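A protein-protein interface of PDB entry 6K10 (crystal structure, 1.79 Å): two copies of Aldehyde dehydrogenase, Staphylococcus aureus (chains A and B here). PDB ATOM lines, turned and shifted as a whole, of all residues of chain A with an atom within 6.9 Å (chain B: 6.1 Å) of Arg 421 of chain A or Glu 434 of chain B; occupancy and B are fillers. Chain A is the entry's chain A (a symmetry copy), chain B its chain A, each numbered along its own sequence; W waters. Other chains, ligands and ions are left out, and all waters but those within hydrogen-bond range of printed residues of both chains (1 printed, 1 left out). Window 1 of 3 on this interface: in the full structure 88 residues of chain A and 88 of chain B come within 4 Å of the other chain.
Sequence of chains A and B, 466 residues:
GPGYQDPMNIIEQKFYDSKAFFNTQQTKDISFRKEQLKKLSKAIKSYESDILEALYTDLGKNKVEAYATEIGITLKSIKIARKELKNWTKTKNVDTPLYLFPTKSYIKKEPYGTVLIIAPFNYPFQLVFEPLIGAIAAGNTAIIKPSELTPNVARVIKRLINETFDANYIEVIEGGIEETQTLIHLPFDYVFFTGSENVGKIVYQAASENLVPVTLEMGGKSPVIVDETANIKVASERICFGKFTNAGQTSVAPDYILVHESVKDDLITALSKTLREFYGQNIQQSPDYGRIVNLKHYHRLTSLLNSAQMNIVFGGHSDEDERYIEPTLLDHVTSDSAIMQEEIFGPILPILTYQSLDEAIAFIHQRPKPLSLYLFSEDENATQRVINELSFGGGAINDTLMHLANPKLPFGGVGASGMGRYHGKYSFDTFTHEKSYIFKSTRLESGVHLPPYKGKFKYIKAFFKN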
ATOM      1  N   TYR A 190      -5.009  13.680 -23.877  1.00  0.00           N
ATOM      2  CA  TYR A 190      -4.938  12.865 -22.673  1.00  0.00           C
ATOM      3  C   TYR A 190      -5.334  11.441 -23.035  1.00  0.00           C
ATOM      4  O   TYR A 190      -6.170  11.225 -23.917  1.00  0.00           O
ATOM      5  CB  TYR A 190      -5.846  13.411 -21.564  1.00  0.00           C
ATOM      6  CG  TYR A 190      -5.416  12.998 -20.178  1.00  0.00           C
ATOM      7  CD1 TYR A 190      -5.801  11.775 -19.645  1.00  0.00           C
ATOM      8  CD2 TYR A 190      -4.618  13.830 -19.404  1.00  0.00           C
ATOM      9  CE1 TYR A 190      -5.401  11.392 -18.378  1.00  0.00           C
ATOM     10  CE2 TYR A 190      -4.215  13.457 -18.137  1.00  0.00           C
ATOM     11  CZ  TYR A 190      -4.608  12.238 -17.628  1.00  0.00           C
ATOM     12  OH  TYR A 190      -4.202  11.874 -16.365  1.00  0.00           O
ATOM     13  N   PHE A 192      -6.564   7.831 -21.099  1.00  0.00           N
ATOM     14  CA  PHE A 192      -7.022   7.147 -19.894  1.00  0.00           C
ATOM     15  C   PHE A 192      -7.156   5.669 -20.221  1.00  0.00           C
ATOM     16  O   PHE A 192      -7.904   5.307 -21.132  1.00  0.00           O
ATOM     17  CB  PHE A 192      -8.355   7.731 -19.400  1.00  0.00           C
ATOM     18  CG  PHE A 192      -8.797   7.199 -18.058  1.00  0.00           C
ATOM     19  CD1 PHE A 192      -9.274   5.900 -17.925  1.00  0.00           C
ATOM     20  CD2 PHE A 192      -8.733   7.995 -16.930  1.00  0.00           C
ATOM     21  CE1 PHE A 192      -9.673   5.413 -16.697  1.00  0.00           C
ATOM     22  CE2 PHE A 192      -9.135   7.510 -15.697  1.00  0.00           C
ATOM     23  CZ  PHE A 192      -9.606   6.217 -15.583  1.00  0.00           C
ATOM     24  N   THR A 215      -3.327   8.502 -17.595  1.00  0.00           N
ATOM     25  CA  THR A 215      -3.686   7.798 -16.376  1.00  0.00           C
ATOM     26  C   THR A 215      -3.760   6.316 -16.711  1.00  0.00           C
ATOM     27  O   THR A 215      -4.413   5.930 -17.686  1.00  0.00           O
ATOM     28  CB  THR A 215      -5.019   8.294 -15.808  1.00  0.00           C
ATOM     29  OG1 THR A 215      -4.828   9.573 -15.194  1.00  0.00           O
ATOM     30  CG2 THR A 215      -5.554   7.316 -14.771  1.00  0.00           C
ATOM     31  N   LEU A 216      -3.071   5.495 -15.925  1.00  0.00           N
ATOM     32  CA  LEU A 216      -3.024   4.054 -16.143  1.00  0.00           C
ATOM     33  C   LEU A 216      -3.560   3.342 -14.909  1.00  0.00           C
ATOM     34  O   LEU A 216      -3.024   3.514 -13.809  1.00  0.00           O
ATOM     35  CB  LEU A 216      -1.599   3.588 -16.450  1.00  0.00           C
ATOM     36  CG  LEU A 216      -0.820   4.315 -17.549  1.00  0.00           C
ATOM     37  CD1 LEU A 216       0.615   3.813 -17.582  1.00  0.00           C
ATOM     38  CD2 LEU A 216      -1.482   4.159 -18.915  1.00  0.00           C
ATOM     39  N   GLU A 217      -4.612   2.551 -15.096  1.00  0.00           N
ATOM     40  CA  GLU A 217      -5.176   1.690 -14.060  1.00  0.00           C
ATOM     41  C   GLU A 217      -4.832   0.260 -14.444  1.00  0.00           C
ATOM     42  O   GLU A 217      -5.436  -0.296 -15.365  1.00  0.00           O
ATOM     43  CB  GLU A 217      -6.693   1.881 -13.949  1.00  0.00           C
ATOM     44  CG  GLU A 217      -7.132   3.276 -13.538  1.00  0.00           C
ATOM     45  CD  GLU A 217      -7.141   3.486 -12.034  1.00  0.00           C
ATOM     46  OE1 GLU A 217      -6.986   2.496 -11.289  1.00  0.00           O
ATOM     47  OE2 GLU A 217      -7.297   4.647 -11.588  1.00  0.00           O
ATOM     48  N   PHE A 392       0.559   0.581  -1.659  1.00  0.00           N
ATOM     49  CA  PHE A 392      -0.375  -0.037  -2.586  1.00  0.00           C
ATOM     50  C   PHE A 392      -1.341   1.046  -3.034  1.00  0.00           C
ATOM     51  O   PHE A 392      -1.374   2.140  -2.468  1.00  0.00           O
ATOM     52  CB  PHE A 392      -1.105  -1.222  -1.942  1.00  0.00           C
ATOM     53  CG  PHE A 392      -1.673  -0.920  -0.582  1.00  0.00           C
ATOM     54  CD1 PHE A 392      -0.903  -1.081   0.559  1.00  0.00           C
ATOM     55  CD2 PHE A 392      -2.977  -0.477  -0.445  1.00  0.00           C
ATOM     56  CE1 PHE A 392      -1.421  -0.805   1.809  1.00  0.00           C
ATOM     57  CE2 PHE A 392      -3.502  -0.198   0.805  1.00  0.00           C
ATOM     58  CZ  PHE A 392      -2.722  -0.364   1.932  1.00  0.00           C
ATOM     59  N   GLY A 393      -2.120   0.738  -4.065  1.00  0.00           N
ATOM     60  CA  GLY A 393      -3.028   1.724  -4.617  1.00  0.00           C
ATOM     61  C   GLY A 393      -4.018   2.257  -3.602  1.00  0.00           C
ATOM     62  O   GLY A 393      -4.048   3.456  -3.312  1.00  0.00           O
ATOM     63  N   GLY A 394      -4.830   1.360  -3.057  1.00  0.00           N
ATOM     64  CA  GLY A 394      -5.778   1.681  -2.004  1.00  0.00           C
ATOM     65  C   GLY A 394      -6.266   0.381  -1.411  1.00  0.00           C
ATOM     66  O   GLY A 394      -6.000  -0.695  -1.945  1.00  0.00           O
ATOM     67  N   PRO A 410     -10.095   8.802  -3.847  1.00  0.00           N
ATOM     68  CA  PRO A 410      -9.477   8.559  -5.155  1.00  0.00           C
ATOM     69  C   PRO A 410      -9.174   7.082  -5.343  1.00  0.00           C
ATOM     70  O   PRO A 410      -8.796   6.382  -4.403  1.00  0.00           O
ATOM     71  CB  PRO A 410      -8.195   9.400  -5.104  1.00  0.00           C
ATOM     72  CG  PRO A 410      -7.905   9.550  -3.648  1.00  0.00           C
ATOM     73  CD  PRO A 410      -9.249   9.645  -2.989  1.00  0.00           C
ATOM     74  N   PHE A 411      -9.366   6.604  -6.567  1.00  0.00           N
ATOM     75  CA  PHE A 411      -9.144   5.204  -6.905  1.00  0.00           C
ATOM     76  C   PHE A 411      -8.053   5.122  -7.959  1.00  0.00           C
ATOM     77  O   PHE A 411      -8.215   5.647  -9.060  1.00  0.00           O
ATOM     78  CB  PHE A 411     -10.431   4.545  -7.411  1.00  0.00           C
ATOM     79  CG  PHE A 411     -10.214   3.178  -8.002  1.00  0.00           C
ATOM     80  CD1 PHE A 411      -9.472   2.223  -7.321  1.00  0.00           C
ATOM     81  CD2 PHE A 411     -10.735   2.851  -9.244  1.00  0.00           C
ATOM     82  CE1 PHE A 411      -9.265   0.967  -7.867  1.00  0.00           C
ATOM     83  CE2 PHE A 411     -10.531   1.595  -9.793  1.00  0.00           C
ATOM     84  CZ  PHE A 411      -9.794   0.652  -9.102  1.00  0.00           C
ATOM     85  N   GLY A 412      -6.956   4.458  -7.622  1.00  0.00           N
ATOM     86  CA  GLY A 412      -5.844   4.322  -8.548  1.00  0.00           C
ATOM     87  C   GLY A 412      -4.737   3.513  -7.916  1.00  0.00           C
ATOM     88  O   GLY A 412      -4.764   3.207  -6.724  1.00  0.00           O
ATOM     89  N   GLY A 413      -3.753   3.169  -8.745  1.00  0.00           N
ATOM     90  CA  GLY A 413      -2.637   2.355  -8.323  1.00  0.00           C
ATOM     91  C   GLY A 413      -1.376   3.161  -8.066  1.00  0.00           C
ATOM     92  O   GLY A 413      -1.373   4.394  -8.040  1.00  0.00           O
ATOM     93  N   MET A 419      -0.757   4.599 -12.411  1.00  0.00           N
ATOM     94  CA  MET A 419      -0.488   5.989 -12.073  1.00  0.00           C
ATOM     95  C   MET A 419      -1.721   6.810 -12.414  1.00  0.00           C
ATOM     96  O   MET A 419      -2.391   6.550 -13.417  1.00  0.00           O
ATOM     97  CB  MET A 419       0.743   6.526 -12.820  1.00  0.00           C
ATOM     98  CG  MET A 419       0.627   6.455 -14.331  1.00  0.00           C
ATOM     99  SD  MET A 419       2.108   7.024 -15.181  1.00  0.00           S
ATOM    100  CE  MET A 419       3.224   5.663 -14.855  1.00  0.00           C
ATOM    101  N   GLY A 420      -2.026   7.793 -11.576  1.00  0.00           N
ATOM    102  CA  GLY A 420      -3.246   8.560 -11.712  1.00  0.00           C
ATOM    103  C   GLY A 420      -4.391   7.944 -10.929  1.00  0.00           C
ATOM    104  O   GLY A 420      -4.278   6.871 -10.336  1.00  0.00           O
ATOM    105  N   ARG A 421      -5.526   8.643 -10.937  1.00  0.00           N
ATOM    106  CA  ARG A 421      -6.662   8.253 -10.108  1.00  0.00           C
ATOM    107  C   ARG A 421      -7.932   8.901 -10.637  1.00  0.00           C
ATOM    108  O   ARG A 421      -7.880   9.867 -11.396  1.00  0.00           O
ATOM    109  CB  ARG A 421      -6.426   8.643  -8.649  1.00  0.00           C
ATOM    110  CG  ARG A 421      -6.579  10.136  -8.397  1.00  0.00           C
ATOM    111  CD  ARG A 421      -5.265  10.786  -8.011  1.00  0.00           C
ATOM    112  NE  ARG A 421      -5.434  12.196  -7.666  1.00  0.00           N
ATOM    113  CZ  ARG A 421      -5.192  12.694  -6.458  1.00  0.00           C
ATOM    114  NH1 ARG A 421      -5.371  13.986  -6.219  1.00  0.00           N
ATOM    115  NH2 ARG A 421      -4.777  11.892  -5.486  1.00  0.00           N
ATOM    116  N   TYR A 422      -9.077   8.359 -10.225  1.00  0.00           N
ATOM    117  CA  TYR A 422     -10.369   8.923 -10.618  1.00  0.00           C
ATOM    118  C   TYR A 422     -11.430   8.491  -9.611  1.00  0.00           C
ATOM    119  O   TYR A 422     -11.106   8.052  -8.504  1.00  0.00           O
ATOM    120  CB  TYR A 422     -10.727   8.552 -12.066  1.00  0.00           C
ATOM    121  CG  TYR A 422     -11.093   7.104 -12.333  1.00  0.00           C
ATOM    122  CD1 TYR A 422     -10.191   6.073 -12.094  1.00  0.00           C
ATOM    123  CD2 TYR A 422     -12.335   6.767 -12.865  1.00  0.00           C
ATOM    124  CE1 TYR A 422     -10.520   4.751 -12.357  1.00  0.00           C
ATOM    125  CE2 TYR A 422     -12.675   5.447 -13.130  1.00  0.00           C
ATOM    126  CZ  TYR A 422     -11.765   4.444 -12.875  1.00  0.00           C
ATOM    127  OH  TYR A 422     -12.099   3.132 -13.138  1.00  0.00           O
ATOM    128  N   HIS A 423     -12.697   8.603 -10.028  1.00  0.00           N
ATOM    129  CA  HIS A 423     -13.913   8.573  -9.213  1.00  0.00           C
ATOM    130  C   HIS A 423     -14.265   9.949  -8.665  1.00  0.00           C
ATOM    131  O   HIS A 423     -13.394  10.682  -8.181  1.00  0.00           O
ATOM    132  CB  HIS A 423     -13.847   7.579  -8.044  1.00  0.00           C
ATOM    133  CG  HIS A 423     -13.922   6.152  -8.466  1.00  0.00           C
ATOM    134  ND1 HIS A 423     -13.984   5.114  -7.561  1.00  0.00           N
ATOM    135  CD2 HIS A 423     -13.942   5.584  -9.694  1.00  0.00           C
ATOM    136  CE1 HIS A 423     -14.053   3.968  -8.213  1.00  0.00           C
ATOM    137  NE2 HIS A 423     -14.026   4.225  -9.509  1.00  0.00           N
ATOM    138  N   TYR A 426     -12.249  13.404  -8.668  1.00  0.00           N
ATOM    139  CA  TYR A 426     -10.961  13.009  -9.230  1.00  0.00           C
ATOM    140  C   TYR A 426     -11.077  12.639 -10.702  1.00  0.00           C
ATOM    141  O   TYR A 426     -10.111  12.811 -11.461  1.00  0.00           O
ATOM    142  CB  TYR A 426     -10.364  11.852  -8.423  1.00  0.00           C
ATOM    143  CG  TYR A 426     -10.117  12.205  -6.975  1.00  0.00           C
ATOM    144  CD1 TYR A 426      -8.972  12.890  -6.594  1.00  0.00           C
ATOM    145  CD2 TYR A 426     -11.038  11.865  -5.992  1.00  0.00           C
ATOM    146  CE1 TYR A 426      -8.744  13.225  -5.271  1.00  0.00           C
ATOM    147  CE2 TYR A 426     -10.821  12.196  -4.670  1.00  0.00           C
ATOM    148  CZ  TYR A 426      -9.674  12.873  -4.313  1.00  0.00           C
ATOM    149  OH  TYR A 426      -9.458  13.198  -2.994  1.00  0.00           O
ATOM    150  N   SER A 427     -12.241  12.133 -11.124  1.00  0.00           N
ATOM    151  CA  SER A 427     -12.473  11.926 -12.548  1.00  0.00           C
ATOM    152  C   SER A 427     -12.426  13.246 -13.301  1.00  0.00           C
ATOM    153  O   SER A 427     -11.820  13.340 -14.375  1.00  0.00           O
ATOM    154  CB  SER A 427     -13.822  11.236 -12.760  1.00  0.00           C
ATOM    155  OG  SER A 427     -13.804   9.910 -12.249  1.00  0.00           O
ATOM    156  N   ASP A 429     -10.876  16.051 -12.150  1.00  0.00           N
ATOM    157  CA  ASP A 429      -9.497  16.524 -12.036  1.00  0.00           C
ATOM    158  C   ASP A 429      -8.588  15.880 -13.077  1.00  0.00           C
ATOM    159  O   ASP A 429      -7.724  16.547 -13.660  1.00  0.00           O
ATOM    160  CB  ASP A 429      -8.956  16.236 -10.633  1.00  0.00           C
ATOM    161  CG  ASP A 429      -9.686  17.003  -9.547  1.00  0.00           C
ATOM    162  OD1 ASP A 429     -10.404  17.975  -9.862  1.00  0.00           O
ATOM    163  OD2 ASP A 429      -9.544  16.628  -8.360  1.00  0.00           O
ATOM    164  N   THR A 430      -8.772  14.578 -13.321  1.00  0.00           N
ATOM    165  CA  THR A 430      -7.882  13.849 -14.221  1.00  0.00           C
ATOM    166  C   THR A 430      -7.892  14.446 -15.625  1.00  0.00           C
ATOM    167  O   THR A 430      -6.843  14.539 -16.273  1.00  0.00           O
ATOM    168  CB  THR A 430      -8.274  12.368 -14.250  1.00  0.00           C
ATOM    169  OG1 THR A 430      -7.941  11.768 -12.994  1.00  0.00           O
ATOM    170  CG2 THR A 430      -7.555  11.622 -15.366  1.00  0.00           C
ATOM    171  N   ILE B 107      -7.507   8.836   3.773  1.00  0.00           N
ATOM    172  CA  ILE B 107      -6.506   8.969   2.721  1.00  0.00           C
ATOM    173  C   ILE B 107      -5.149   9.086   3.397  1.00  0.00           C
ATOM    174  O   ILE B 107      -4.885  10.067   4.105  1.00  0.00           O
ATOM    175  CB  ILE B 107      -6.765  10.175   1.808  1.00  0.00           C
ATOM    176  CG1 ILE B 107      -8.067   9.969   1.030  1.00  0.00           C
ATOM    177  CG2 ILE B 107      -5.588  10.372   0.856  1.00  0.00           C
ATOM    178  CD1 ILE B 107      -8.452  11.135   0.150  1.00  0.00           C
ATOM    179  N   LYS B 108      -4.297   8.086   3.191  1.00  0.00           N
ATOM    180  CA  LYS B 108      -2.925   8.094   3.677  1.00  0.00           C
ATOM    181  C   LYS B 108      -2.025   8.751   2.639  1.00  0.00           C
ATOM    182  O   LYS B 108      -2.112   8.434   1.449  1.00  0.00           O
ATOM    183  CB  LYS B 108      -2.466   6.660   3.955  1.00  0.00           C
ATOM    184  CG  LYS B 108      -0.962   6.461   4.066  1.00  0.00           C
ATOM    185  CD  LYS B 108      -0.448   6.880   5.428  1.00  0.00           C
ATOM    186  CE  LYS B 108       0.966   6.368   5.656  1.00  0.00           C
ATOM    187  NZ  LYS B 108       1.399   6.527   7.070  1.00  0.00           N
ATOM    188  N   LYS B 109      -1.173   9.671   3.084  1.00  0.00           N
ATOM    189  CA  LYS B 109      -0.175  10.292   2.219  1.00  0.00           C
ATOM    190  C   LYS B 109       1.150   9.566   2.418  1.00  0.00           C
ATOM    191  O   LYS B 109       1.680   9.534   3.533  1.00  0.00           O
ATOM    192  CB  LYS B 109      -0.023  11.783   2.523  1.00  0.00           C
ATOM    193  CG  LYS B 109      -1.012  12.680   1.794  1.00  0.00           C
ATOM    194  CD  LYS B 109      -2.141  13.116   2.710  1.00  0.00           C
ATOM    195  N   GLU B 110       1.680   8.981   1.348  1.00  0.00           N
ATOM    196  CA  GLU B 110       2.881   8.170   1.466  1.00  0.00           C
ATOM    197  C   GLU B 110       3.820   8.443   0.298  1.00  0.00           C
ATOM    198  O   GLU B 110       3.376   8.866  -0.776  1.00  0.00           O
ATOM    199  CB  GLU B 110       2.546   6.671   1.527  1.00  0.00           C
ATOM    200  CG  GLU B 110       1.995   6.081   0.239  1.00  0.00           C
ATOM    201  CD  GLU B 110       1.687   4.601   0.370  1.00  0.00           C
ATOM    202  OE1 GLU B 110       1.780   4.069   1.495  1.00  0.00           O
ATOM    203  OE2 GLU B 110       1.352   3.967  -0.653  1.00  0.00           O
ATOM    204  N   TYR B 112       6.629   7.798  -2.814  1.00  0.00           N
ATOM    205  CA  TYR B 112       6.837   6.850  -3.901  1.00  0.00           C
ATOM    206  C   TYR B 112       8.018   5.933  -3.622  1.00  0.00           C
ATOM    207  O   TYR B 112       7.983   4.746  -3.965  1.00  0.00           O
ATOM    208  CB  TYR B 112       7.064   7.600  -5.213  1.00  0.00           C
ATOM    209  CG  TYR B 112       5.808   8.143  -5.847  1.00  0.00           C
ATOM    210  CD1 TYR B 112       4.933   7.303  -6.521  1.00  0.00           C
ATOM    211  CD2 TYR B 112       5.501   9.494  -5.778  1.00  0.00           C
ATOM    212  CE1 TYR B 112       3.785   7.792  -7.107  1.00  0.00           C
ATOM    213  CE2 TYR B 112       4.354   9.995  -6.361  1.00  0.00           C
ATOM    214  CZ  TYR B 112       3.499   9.139  -7.023  1.00  0.00           C
ATOM    215  OH  TYR B 112       2.356   9.627  -7.609  1.00  0.00           O
ATOM    216  N   LYS B 425       2.679  23.288  -1.549  1.00  0.00           N
ATOM    217  CA  LYS B 425       2.163  21.948  -1.286  1.00  0.00           C
ATOM    218  C   LYS B 425       2.149  21.084  -2.543  1.00  0.00           C
ATOM    219  O   LYS B 425       2.202  19.850  -2.443  1.00  0.00           O
ATOM    220  CB  LYS B 425       0.762  22.041  -0.676  1.00  0.00           C
ATOM    221  CG  LYS B 425       0.184  20.697  -0.253  1.00  0.00           C
ATOM    222  CD  LYS B 425      -1.141  20.823   0.472  1.00  0.00           C
ATOM    223  CE  LYS B 425      -1.637  19.453   0.914  1.00  0.00           C
ATOM    224  NZ  LYS B 425      -2.058  18.600  -0.239  1.00  0.00           N
ATOM    225  N   ASP B 429       2.735  17.218  -3.026  1.00  0.00           N
ATOM    226  CA  ASP B 429       1.782  16.357  -3.725  1.00  0.00           C
ATOM    227  C   ASP B 429       2.447  15.570  -4.849  1.00  0.00           C
ATOM    228  O   ASP B 429       2.152  14.385  -5.049  1.00  0.00           O
ATOM    229  CB  ASP B 429       0.635  17.196  -4.294  1.00  0.00           C
ATOM    230  CG  ASP B 429      -0.207  17.858  -3.220  1.00  0.00           C
ATOM    231  OD1 ASP B 429      -0.117  17.458  -2.040  1.00  0.00           O
ATOM    232  OD2 ASP B 429      -0.967  18.796  -3.556  1.00  0.00           O
ATOM    233  N   THR B 432       4.052  12.438  -3.724  1.00  0.00           N
ATOM    234  CA  THR B 432       3.204  11.733  -2.774  1.00  0.00           C
ATOM    235  C   THR B 432       2.200  10.878  -3.530  1.00  0.00           C
ATOM    236  O   THR B 432       1.561  11.356  -4.473  1.00  0.00           O
ATOM    237  CB  THR B 432       2.467  12.722  -1.864  1.00  0.00           C
ATOM    238  OG1 THR B 432       3.406  13.356  -0.986  1.00  0.00           O
ATOM    239  CG2 THR B 432       1.391  12.017  -1.040  1.00  0.00           C
ATOM    240  N   HIS B 433       2.068   9.619  -3.129  1.00  0.00           N
ATOM    241  CA  HIS B 433       0.930   8.818  -3.546  1.00  0.00           C
ATOM    242  C   HIS B 433      -0.154   8.920  -2.485  1.00  0.00           C
ATOM    243  O   HIS B 433       0.098   8.653  -1.306  1.00  0.00           O
ATOM    244  CB  HIS B 433       1.297   7.353  -3.754  1.00  0.00           C
ATOM    245  CG  HIS B 433       0.098   6.478  -3.945  1.00  0.00           C
ATOM    246  ND1 HIS B 433      -0.156   5.373  -3.161  1.00  0.00           N
ATOM    247  CD2 HIS B 433      -0.938   6.573  -4.810  1.00  0.00           C
ATOM    248  CE1 HIS B 433      -1.291   4.817  -3.548  1.00  0.00           C
ATOM    249  NE2 HIS B 433      -1.785   5.524  -4.547  1.00  0.00           N
ATOM    250  N   GLU B 434      -1.351   9.308  -2.903  1.00  0.00           N
ATOM    251  CA  GLU B 434      -2.491   9.375  -2.001  1.00  0.00           C
ATOM    252  C   GLU B 434      -3.184   8.018  -1.999  1.00  0.00           C
ATOM    253  O   GLU B 434      -3.674   7.562  -3.038  1.00  0.00           O
ATOM    254  CB  GLU B 434      -3.440  10.496  -2.417  1.00  0.00           C
ATOM    255  CG  GLU B 434      -2.864  11.871  -2.110  1.00  0.00           C
ATOM    256  CD  GLU B 434      -3.882  12.981  -2.236  1.00  0.00           C
ATOM    257  OE1 GLU B 434      -4.884  12.788  -2.953  1.00  0.00           O
ATOM    258  OE2 GLU B 434      -3.677  14.045  -1.616  1.00  0.00           O
ATOM    259  N   LYS B 435      -3.206   7.372  -0.840  1.00  0.00           N
ATOM    260  CA  LYS B 435      -3.648   5.986  -0.709  1.00  0.00           C
ATOM    261  C   LYS B 435      -4.964   5.964   0.059  1.00  0.00           C
ATOM    262  O   LYS B 435      -4.985   6.137   1.282  1.00  0.00           O
ATOM    263  CB  LYS B 435      -2.576   5.151  -0.016  1.00  0.00           C
ATOM    264  CG  LYS B 435      -2.886   3.667   0.070  1.00  0.00           C
ATOM    265  CD  LYS B 435      -1.664   2.886   0.544  1.00  0.00           C
ATOM    266  CE  LYS B 435      -1.422   3.069   2.033  1.00  0.00           C
ATOM    267  NZ  LYS B 435      -0.101   2.515   2.453  1.00  0.00           N
ATOM    268  N   SER B 436      -6.059   5.753  -0.662  1.00  0.00           N
ATOM    269  CA  SER B 436      -7.363   5.640  -0.026  1.00  0.00           C
ATOM    270  C   SER B 436      -7.468   4.324   0.725  1.00  0.00           C
ATOM    271  O   SER B 436      -7.009   3.284   0.250  1.00  0.00           O
ATOM    272  CB  SER B 436      -8.476   5.713  -1.069  1.00  0.00           C
ATOM    273  OG  SER B 436      -8.474   6.957  -1.736  1.00  0.00           O
HETATM  274  O   HOH W   1      -6.156   5.082  -3.578  1.00  0.00           O
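Arg 421 of chain A touches just one residue of chain B: Glu 434. Of chain A, only Arg 421 comes within 4 Å of Glu 434 of chain B. Printed residues of chain B within 4 Å of Tyr 426 of chain A: Ile 107. Of the printed residues of chain B, Gly 413 of chain A touches His 433 (3.7 Å). Of the printed residues of chain A, His 433 of chain B touches Phe 392, Gly 393 and Gly 413. Of the printed residues of chain A, Lys 435 of chain B touches Phe 392 (3.1 Å) and Gly 393 (3.6 Å). Of the printed residues of chain A, Ser 436 of chain B touches Gly 394 and Pro 410. Phe 411 of chain A touches none of the printed residues of chain B.
Water W1 lies within hydrogen-bond range of O of Gly 393 of chain A (2.7 Å), N of Ser 436 of chain B (3.0 Å) and O of Pro 410 of chain A (3.1 Å).
The backbone carbonyl oxygen of Lys 108 of chain B sits at hydrogen-bond distance from the backbone NH of Lys 435 of chain B (2.8 Å). The backbone NH (N) of His 433 of chain B sits at hydrogen-bond distance from the backbone carbonyl oxygen (O) of Glu 110 of chain B (2.8 Å). The side-chain amino group (NZ) of Lys 435 of chain B is in salt-bridge range of the side-chain carboxylate (OE1) of Glu 110 of chain B, 2.6 Å away. The backbone carbonyl oxygen (O) of Arg 421 of chain A is in hydrogen-bond range of the side-chain hydroxyl (OG1) of Thr 430 of chain A, 2.5 Å away. The backbone carbonyl oxygen (O) of Tyr 426 of chain A is in hydrogen-bond range of the side-chain hydroxyl (OG1) of Thr 430 of chain A (2.9 Å).
Hydrophobic or aromatic side chains of chain B that line the printed part of chain A: Ile 107 and His 433. Of the 21 printed residues of chain A, 7 touch a printed residue of chain B. Hydrophobic or aromatic side chains of chain A that line the printed part of chain B: Phe 392, Pro 410 and Tyr 426. Among the printed residues, Asp or Glu carboxylates within 4 Å of a Lys or Arg side-chain nitrogen of the other chain: Arg 421 of chain A with Glu 434 of chain B.
The backbone carbonyl oxygen (O) of Gly 393 of chain A sits close to a ring nitrogen (NE2) of His 433 of chain B (3.3 Å). The side-chain carboxylate of Glu 434 of chain B lies within salt-bridge range of the guanidinium group of Arg 421 of chain A (2.7 Å). The side-chain hydroxyl (OG) of Ser 436 of chain B sits at hydrogen-bond distance from the backbone carbonyl oxygen (O) of Pro 410 of chain A, at 2.7 Å.
Position printed for both chains: 429. Of the 11 pairs that touch across the chains among the printed residues, none has its exchanged pair printed and touching as well.
N of Phe 392 of chain A touches OE2 of Glu 110 of chain B, 3.6 Å away. Phe 392 of chain A touches His 433 of chain B. CD of Lys 435 of chain B touches O of Phe 392 of chain A, at 3.1 Å. Gly 393 of chain A touches Lys 435 of chain B (O to CG, 3.6 Å). Ser 436 of chain B touches Gly 394 of chain A (O to CA, 3.0 Å). Ile 107 of chain B touches Pro 410 of chain A. Gly 413 of chain A touches His 433 of chain B (O to NE2, 3.7 Å). CD1 of Ile 107 of chain B touches OH of Tyr 426 of chain A (3.9 Å).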
